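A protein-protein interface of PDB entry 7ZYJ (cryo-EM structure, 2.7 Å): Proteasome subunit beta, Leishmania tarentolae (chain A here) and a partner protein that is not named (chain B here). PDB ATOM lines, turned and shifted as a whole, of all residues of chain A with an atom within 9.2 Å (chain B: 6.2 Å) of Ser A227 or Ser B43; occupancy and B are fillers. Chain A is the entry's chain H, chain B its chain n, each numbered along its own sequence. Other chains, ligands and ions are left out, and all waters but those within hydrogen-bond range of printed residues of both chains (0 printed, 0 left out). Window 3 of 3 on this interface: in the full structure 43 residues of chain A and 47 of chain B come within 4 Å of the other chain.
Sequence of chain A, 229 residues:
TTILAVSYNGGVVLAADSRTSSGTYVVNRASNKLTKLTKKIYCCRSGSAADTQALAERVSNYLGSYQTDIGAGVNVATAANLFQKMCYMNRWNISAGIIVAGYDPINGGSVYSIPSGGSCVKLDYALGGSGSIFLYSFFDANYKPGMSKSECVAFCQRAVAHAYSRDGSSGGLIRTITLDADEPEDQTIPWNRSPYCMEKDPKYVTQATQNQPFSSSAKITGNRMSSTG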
ATOM      1  N   PRO A 213     -19.116  -6.628 -27.548  1.00  0.00           N
ATOM      2  CA  PRO A 213     -19.330  -7.888 -26.833  1.00  0.00           C
ATOM      3  C   PRO A 213     -18.590  -7.872 -25.506  1.00  0.00           C
ATOM      4  O   PRO A 213     -17.559  -7.212 -25.353  1.00  0.00           O
ATOM      5  CB  PRO A 213     -18.750  -8.945 -27.781  1.00  0.00           C
ATOM      6  CG  PRO A 213     -18.645  -8.272 -29.111  1.00  0.00           C
ATOM      7  CD  PRO A 213     -18.400  -6.826 -28.817  1.00  0.00           C
ATOM      8  N   PHE A 214     -19.130  -8.603 -24.535  1.00  0.00           N
ATOM      9  CA  PHE A 214     -18.471  -8.715 -23.238  1.00  0.00           C
ATOM     10  C   PHE A 214     -17.172  -9.489 -23.415  1.00  0.00           C
ATOM     11  O   PHE A 214     -17.186 -10.660 -23.806  1.00  0.00           O
ATOM     12  CB  PHE A 214     -19.392  -9.397 -22.231  1.00  0.00           C
ATOM     13  CG  PHE A 214     -18.953  -9.233 -20.806  1.00  0.00           C
ATOM     14  CD1 PHE A 214     -18.606  -7.985 -20.316  1.00  0.00           C
ATOM     15  CD2 PHE A 214     -18.889 -10.322 -19.955  1.00  0.00           C
ATOM     16  CE1 PHE A 214     -18.203  -7.827 -19.006  1.00  0.00           C
ATOM     17  CE2 PHE A 214     -18.485 -10.168 -18.644  1.00  0.00           C
ATOM     18  CZ  PHE A 214     -18.142  -8.918 -18.169  1.00  0.00           C
ATOM     19  N   ARG A 224     -21.421  -6.691 -31.534  1.00  0.00           N
ATOM     20  CA  ARG A 224     -21.999  -8.000 -31.248  1.00  0.00           C
ATOM     21  C   ARG A 224     -23.307  -8.123 -32.018  1.00  0.00           C
ATOM     22  O   ARG A 224     -24.276  -7.412 -31.730  1.00  0.00           O
ATOM     23  CB  ARG A 224     -22.220  -8.173 -29.748  1.00  0.00           C
ATOM     24  CG  ARG A 224     -22.766  -9.531 -29.351  1.00  0.00           C
ATOM     25  CD  ARG A 224     -23.190  -9.543 -27.893  1.00  0.00           C
ATOM     26  NE  ARG A 224     -23.843 -10.792 -27.523  1.00  0.00           N
ATOM     27  CZ  ARG A 224     -24.786 -10.897 -26.596  1.00  0.00           C
ATOM     28  NH1 ARG A 224     -25.212  -9.841 -25.923  1.00  0.00           N
ATOM     29  NH2 ARG A 224     -25.314 -12.089 -26.340  1.00  0.00           N
ATOM     30  N   MET A 225     -23.340  -9.025 -32.998  1.00  0.00           N
ATOM     31  CA  MET A 225     -24.504  -9.197 -33.856  1.00  0.00           C
ATOM     32  C   MET A 225     -25.171 -10.554 -33.684  1.00  0.00           C
ATOM     33  O   MET A 225     -26.049 -10.906 -34.477  1.00  0.00           O
ATOM     34  CB  MET A 225     -24.114  -8.984 -35.320  1.00  0.00           C
ATOM     35  CG  MET A 225     -23.701  -7.560 -35.644  1.00  0.00           C
ATOM     36  SD  MET A 225     -23.171  -7.359 -37.353  1.00  0.00           S
ATOM     37  CE  MET A 225     -24.733  -7.538 -38.209  1.00  0.00           C
ATOM     38  N   SER A 226     -24.780 -11.324 -32.671  1.00  0.00           N
ATOM     39  CA  SER A 226     -25.402 -12.612 -32.410  1.00  0.00           C
ATOM     40  C   SER A 226     -25.410 -12.861 -30.909  1.00  0.00           C
ATOM     41  O   SER A 226     -24.533 -12.387 -30.183  1.00  0.00           O
ATOM     42  CB  SER A 226     -24.675 -13.750 -33.134  1.00  0.00           C
ATOM     43  OG  SER A 226     -25.509 -14.887 -33.259  1.00  0.00           O
ATOM     44  N   SER A 227     -26.418 -13.607 -30.453  1.00  0.00           N
ATOM     45  CA  SER A 227     -26.515 -13.931 -29.034  1.00  0.00           C
ATOM     46  C   SER A 227     -25.353 -14.813 -28.594  1.00  0.00           C
ATOM     47  O   SER A 227     -24.729 -14.565 -27.556  1.00  0.00           O
ATOM     48  CB  SER A 227     -27.850 -14.611 -28.740  1.00  0.00           C
ATOM     49  OG  SER A 227     -28.898 -13.661 -28.653  1.00  0.00           O
ATOM     50  N   THR A 228     -25.051 -15.854 -29.375  1.00  0.00           N
ATOM     51  CA  THR A 228     -23.926 -16.722 -29.046  1.00  0.00           C
ATOM     52  C   THR A 228     -22.598 -15.983 -29.142  1.00  0.00           C
ATOM     53  O   THR A 228     -21.724 -16.164 -28.287  1.00  0.00           O
ATOM     54  CB  THR A 228     -23.919 -17.944 -29.965  1.00  0.00           C
ATOM     55  OG1 THR A 228     -23.828 -17.517 -31.329  1.00  0.00           O
ATOM     56  CG2 THR A 228     -25.191 -18.758 -29.776  1.00  0.00           C
ATOM     57  N   GLY A 229     -22.430 -15.149 -30.163  1.00  0.00           N
ATOM     58  CA  GLY A 229     -21.203 -14.394 -30.337  1.00  0.00           C
ATOM     59  C   GLY A 229     -21.379 -12.907 -30.097  1.00  0.00           C
ATOM     60  O   GLY A 229     -20.817 -12.351 -29.153  1.00  0.00           O
ATOM     61  N   LEU B  40     -28.115  -6.011 -28.161  1.00  0.00           N
ATOM     62  CA  LEU B  40     -28.429  -7.321 -27.612  1.00  0.00           C
ATOM     63  C   LEU B  40     -28.283  -7.285 -26.098  1.00  0.00           C
ATOM     64  O   LEU B  40     -27.237  -6.881 -25.580  1.00  0.00           O
ATOM     65  CB  LEU B  40     -27.516  -8.397 -28.203  1.00  0.00           C
ATOM     66  CG  LEU B  40     -27.679  -8.668 -29.696  1.00  0.00           C
ATOM     67  CD1 LEU B  40     -26.786  -9.813 -30.127  1.00  0.00           C
ATOM     68  CD2 LEU B  40     -29.128  -8.962 -30.029  1.00  0.00           C
ATOM     69  N   LEU B  41     -29.333  -7.700 -25.398  1.00  0.00           N
ATOM     70  CA  LEU B  41     -29.333  -7.809 -23.948  1.00  0.00           C
ATOM     71  C   LEU B  41     -29.389  -9.281 -23.568  1.00  0.00           C
ATOM     72  O   LEU B  41     -30.289 -10.012 -24.008  1.00  0.00           O
ATOM     73  CB  LEU B  41     -30.515  -7.056 -23.337  1.00  0.00           C
ATOM     74  CG  LEU B  41     -30.607  -5.560 -23.637  1.00  0.00           C
ATOM     75  CD1 LEU B  41     -31.888  -4.988 -23.057  1.00  0.00           C
ATOM     76  CD2 LEU B  41     -29.392  -4.826 -23.097  1.00  0.00           C
ATOM     77  N   GLY B  42     -28.423  -9.709 -22.762  1.00  0.00           N
ATOM     78  CA  GLY B  42     -28.303 -11.084 -22.362  1.00  0.00           C
ATOM     79  C   GLY B  42     -27.995 -11.970 -23.557  1.00  0.00           C
ATOM     80  O   GLY B  42     -27.454 -11.538 -24.577  1.00  0.00           O
ATOM     81  N   SER B  43     -28.356 -13.240 -23.411  1.00  0.00           N
ATOM     82  CA  SER B  43     -28.257 -14.206 -24.492  1.00  0.00           C
ATOM     83  C   SER B  43     -29.609 -14.513 -25.113  1.00  0.00           C
ATOM     84  O   SER B  43     -29.715 -15.439 -25.923  1.00  0.00           O
ATOM     85  CB  SER B  43     -27.605 -15.496 -23.991  1.00  0.00           C
ATOM     86  OG  SER B  43     -28.436 -16.153 -23.052  1.00  0.00           O
ATOM     87  N   HIS B  44     -30.646 -13.758 -24.752  1.00  0.00           N
ATOM     88  CA  HIS B  44     -31.999 -14.046 -25.202  1.00  0.00           C
ATOM     89  C   HIS B  44     -32.772 -12.846 -25.726  1.00  0.00           C
ATOM     90  O   HIS B  44     -33.812 -13.054 -26.362  1.00  0.00           O
ATOM     91  CB  HIS B  44     -32.820 -14.680 -24.068  1.00  0.00           C
ATOM     92  CG  HIS B  44     -32.277 -15.987 -23.583  1.00  0.00           C
ATOM     93  ND1 HIS B  44     -32.168 -17.095 -24.393  1.00  0.00           N
ATOM     94  CD2 HIS B  44     -31.823 -16.365 -22.364  1.00  0.00           C
ATOM     95  CE1 HIS B  44     -31.663 -18.099 -23.698  1.00  0.00           C
ATOM     96  NE2 HIS B  44     -31.446 -17.682 -22.464  1.00  0.00           N
ATOM     97  N   SER B  45     -32.328 -11.612 -25.489  1.00  0.00           N
ATOM     98  CA  SER B  45     -33.185 -10.469 -25.760  1.00  0.00           C
ATOM     99  C   SER B  45     -32.456  -9.402 -26.563  1.00  0.00           C
ATOM    100  O   SER B  45     -31.231  -9.402 -26.682  1.00  0.00           O
ATOM    101  CB  SER B  45     -33.725  -9.870 -24.457  1.00  0.00           C
ATOM    102  OG  SER B  45     -32.680  -9.336 -23.669  1.00  0.00           O
ATOM    103  N   GLU B  64     -27.607  -4.308 -19.071  1.00  0.00           N
ATOM    104  CA  GLU B  64     -26.682  -5.378 -19.428  1.00  0.00           C
ATOM    105  C   GLU B  64     -25.736  -5.719 -18.284  1.00  0.00           C
ATOM    106  O   GLU B  64     -25.388  -6.892 -18.107  1.00  0.00           O
ATOM    107  CB  GLU B  64     -25.888  -4.990 -20.675  1.00  0.00           C
ATOM    108  CG  GLU B  64     -24.928  -6.061 -21.173  1.00  0.00           C
ATOM    109  CD  GLU B  64     -25.616  -7.386 -21.443  1.00  0.00           C
ATOM    110  OE1 GLU B  64     -25.521  -8.294 -20.590  1.00  0.00           O
ATOM    111  OE2 GLU B  64     -26.252  -7.521 -22.509  1.00  0.00           O
ATOM    112  N   ILE B  67     -27.680  -8.098 -15.803  1.00  0.00           N
ATOM    113  CA  ILE B  67     -27.847  -9.490 -16.211  1.00  0.00           C
ATOM    114  C   ILE B  67     -26.553 -10.271 -16.020  1.00  0.00           C
ATOM    115  O   ILE B  67     -26.538 -11.340 -15.397  1.00  0.00           O
ATOM    116  CB  ILE B  67     -28.326  -9.560 -17.672  1.00  0.00           C
ATOM    117  CG1 ILE B  67     -29.648  -8.816 -17.846  1.00  0.00           C
ATOM    118  CG2 ILE B  67     -28.462 -11.006 -18.122  1.00  0.00           C
ATOM    119  CD1 ILE B  67     -30.068  -8.675 -19.289  1.00  0.00           C
ATOM    120  N   LYS B  71     -25.766 -13.302 -13.344  1.00  0.00           N
ATOM    121  CA  LYS B  71     -25.420 -14.634 -13.829  1.00  0.00           C
ATOM    122  C   LYS B  71     -24.054 -15.082 -13.321  1.00  0.00           C
ATOM    123  O   LYS B  71     -23.863 -16.267 -13.027  1.00  0.00           O
ATOM    124  CB  LYS B  71     -25.454 -14.662 -15.356  1.00  0.00           C
ATOM    125  CG  LYS B  71     -25.147 -16.022 -15.959  1.00  0.00           C
ATOM    126  CD  LYS B  71     -25.324 -16.014 -17.466  1.00  0.00           C
ATOM    127  CE  LYS B  71     -24.200 -15.253 -18.148  1.00  0.00           C
ATOM    128  NZ  LYS B  71     -24.292 -15.333 -19.632  1.00  0.00           N
ATOM    129  N   GLU B  78     -29.868 -17.496 -16.188  1.00  0.00           N
ATOM    130  CA  GLU B  78     -29.908 -16.158 -16.759  1.00  0.00           C
ATOM    131  C   GLU B  78     -31.335 -15.620 -16.734  1.00  0.00           C
ATOM    132  O   GLU B  78     -32.308 -16.369 -16.856  1.00  0.00           O
ATOM    133  CB  GLU B  78     -29.366 -16.180 -18.187  1.00  0.00           C
ATOM    134  CG  GLU B  78     -29.229 -14.818 -18.835  1.00  0.00           C
ATOM    135  CD  GLU B  78     -28.668 -14.903 -20.236  1.00  0.00           C
ATOM    136  OE1 GLU B  78     -28.310 -16.019 -20.669  1.00  0.00           O
ATOM    137  OE2 GLU B  78     -28.587 -13.858 -20.910  1.00  0.00           O
ATOM    138  N   VAL B 111     -36.727 -14.249 -26.780  1.00  0.00           N
ATOM    139  CA  VAL B 111     -37.228 -15.616 -26.871  1.00  0.00           C
ATOM    140  C   VAL B 111     -36.394 -16.490 -25.945  1.00  0.00           C
ATOM    141  O   VAL B 111     -35.163 -16.385 -25.921  1.00  0.00           O
ATOM    142  CB  VAL B 111     -37.180 -16.159 -28.316  1.00  0.00           C
ATOM    143  CG1 VAL B 111     -37.374 -17.666 -28.326  1.00  0.00           C
ATOM    144  CG2 VAL B 111     -38.233 -15.491 -29.185  1.00  0.00           C
ATOM    145  N   ASP B 192     -32.899 -20.368 -30.841  1.00  0.00           N
ATOM    146  CA  ASP B 192     -31.453 -20.436 -30.659  1.00  0.00           C
ATOM    147  C   ASP B 192     -30.893 -19.150 -30.068  1.00  0.00           C
ATOM    148  O   ASP B 192     -29.858 -19.180 -29.392  1.00  0.00           O
ATOM    149  CB  ASP B 192     -30.771 -20.743 -31.992  1.00  0.00           C
ATOM    150  CG  ASP B 192     -31.266 -19.856 -33.116  1.00  0.00           C
ATOM    151  OD1 ASP B 192     -32.425 -20.033 -33.547  1.00  0.00           O
ATOM    152  OD2 ASP B 192     -30.498 -18.979 -33.565  1.00  0.00           O
ATOM    153  N   GLY B 193     -31.546 -18.027 -30.306  1.00  0.00           N
ATOM    154  CA  GLY B 193     -31.074 -16.753 -29.800  1.00  0.00           C
ATOM    155  C   GLY B 193     -31.470 -15.634 -30.740  1.00  0.00           C
ATOM    156  O   GLY B 193     -32.196 -15.829 -31.709  1.00  0.00           O
ATOM    157  N   VAL B 194     -30.968 -14.446 -30.425  1.00  0.00           N
ATOM    158  CA  VAL B 194     -31.249 -13.265 -31.231  1.00  0.00           C
ATOM    159  C   VAL B 194     -30.087 -13.017 -32.181  1.00  0.00           C
ATOM    160  O   VAL B 194     -28.917 -13.047 -31.781  1.00  0.00           O
ATOM    161  CB  VAL B 194     -31.513 -12.043 -30.336  1.00  0.00           C
ATOM    162  CG1 VAL B 194     -32.000 -10.871 -31.173  1.00  0.00           C
ATOM    163  CG2 VAL B 194     -32.522 -12.388 -29.261  1.00  0.00           C
ATOM    164  N   ARG B 195     -30.410 -12.771 -33.447  1.00  0.00           N
ATOM    165  CA  ARG B 195     -29.410 -12.562 -34.485  1.00  0.00           C
ATOM    166  C   ARG B 195     -29.722 -11.263 -35.208  1.00  0.00           C
ATOM    167  O   ARG B 195     -30.841 -11.075 -35.689  1.00  0.00           O
ATOM    168  CB  ARG B 195     -29.391 -13.735 -35.468  1.00  0.00           C
ATOM    169  CG  ARG B 195     -28.285 -13.672 -36.499  1.00  0.00           C
ATOM    170  CD  ARG B 195     -28.338 -14.881 -37.414  1.00  0.00           C
ATOM    171  NE  ARG B 195     -28.074 -16.117 -36.686  1.00  0.00           N
ATOM    172  CZ  ARG B 195     -26.863 -16.590 -36.426  1.00  0.00           C
ATOM    173  NH1 ARG B 195     -25.772 -15.951 -36.816  1.00  0.00           N
ATOM    174  NH2 ARG B 195     -26.742 -17.732 -35.754  1.00  0.00           N
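N of Val B194 lies within hydrogen-bond range of OG of Ser A227, at 2.8 Å.
The backbone carbonyl oxygen (O) of Ser B43 lies within hydrogen-bond range of the side-chain hydroxyl (OG) of Ser A227, 3.4 Å away.
O of Gly B42 sits at hydrogen-bond distance from NH2 of Arg A224, at 2.8 Å.
The backbone NH (N) of Ser B43 is in hydrogen-bond range of the side-chain carboxylate (OE2) of Glu B78 (2.6 Å).
The side-chain hydroxyl (OG) of Ser B43 is in hydrogen-bond range of a ring nitrogen (NE2) of His B44, at 3.4 Å.
The backbone NH (N) of Gly B42 sits at hydrogen-bond distance from the side-chain carboxylate (OE2) of Glu B64.
NE of Arg A224 sits at hydrogen-bond distance from O of Ser A226 (3.2 Å).
NH2 of Arg A224 sits at hydrogen-bond distance from O of Ser A227, 2.8 Å away.
Arg A224 touches Leu B40.
Leu B40 touches Met A225 (CD1 to C, 3.98 Å).
Met A225 touches Arg B195.
CD1 of Leu B40 touches O of Ser A226, 3.4 Å away.
Ser A226 touches Val B194.
Ser A226 touches Arg B195 (OG to NH1, 3.7 Å).
Ser A227 touches Leu B40.
Gly B193 touches Ser A227.
Printed residues of chain B within 4 Å of Ser A227: Leu B40, Ser B43, Gly B193 and Val B194.
Of chain A, only Ser A227 (3.4 Å) comes within 4 Å of Ser B43.
Of chain A, only Arg A224 (2.8 Å) comes within 4 Å of Gly B42.
Of the printed residues of chain A, Val B194 touches Ser A226 (3.6 Å) and Ser A227 (2.8 Å).
Of the printed residues of chain B, Met A225 touches Leu B40 (3.98 Å) and Arg B195 (3.7 Å).
Printed residues of chain A within 4 Å of Leu B40: Arg A224, Met A225, Ser A226 and Ser A227.
Of the printed residues of chain B, Ser A226 touches Leu B40, Val B194 and Arg B195.
Of the printed residues of chain A, Gly B193 touches Ser A227 (3.9 Å).
Ser B45 touches none of the printed residues of chain A.
Glu B78 touches none of the printed residues of chain A.
The nearest residue of chain A that does not touch Ser B43 is Arg A224 (4.1 Å).
The nearest printed residue of chain A that does not touch Gly B193 is Thr A228 (6.1 Å).
Of the 8 printed residues of chain A, 4 touch a printed residue of chain B.
Printed residues of chain A that touch a printed residue of chain B: Arg A224, Met A225, Ser A226 and Ser A227.
Printed residues of chain B that touch a printed residue of chain A: Leu B40, Gly B42, Ser B43, Gly B193, Val B194 and Arg B195.
Among the printed residues, 11 pairs touch across the chains.
Among the printed residues, no Asp or Glu carboxylate lies within 4 Å of a Lys or Arg side-chain nitrogen of the other chain.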
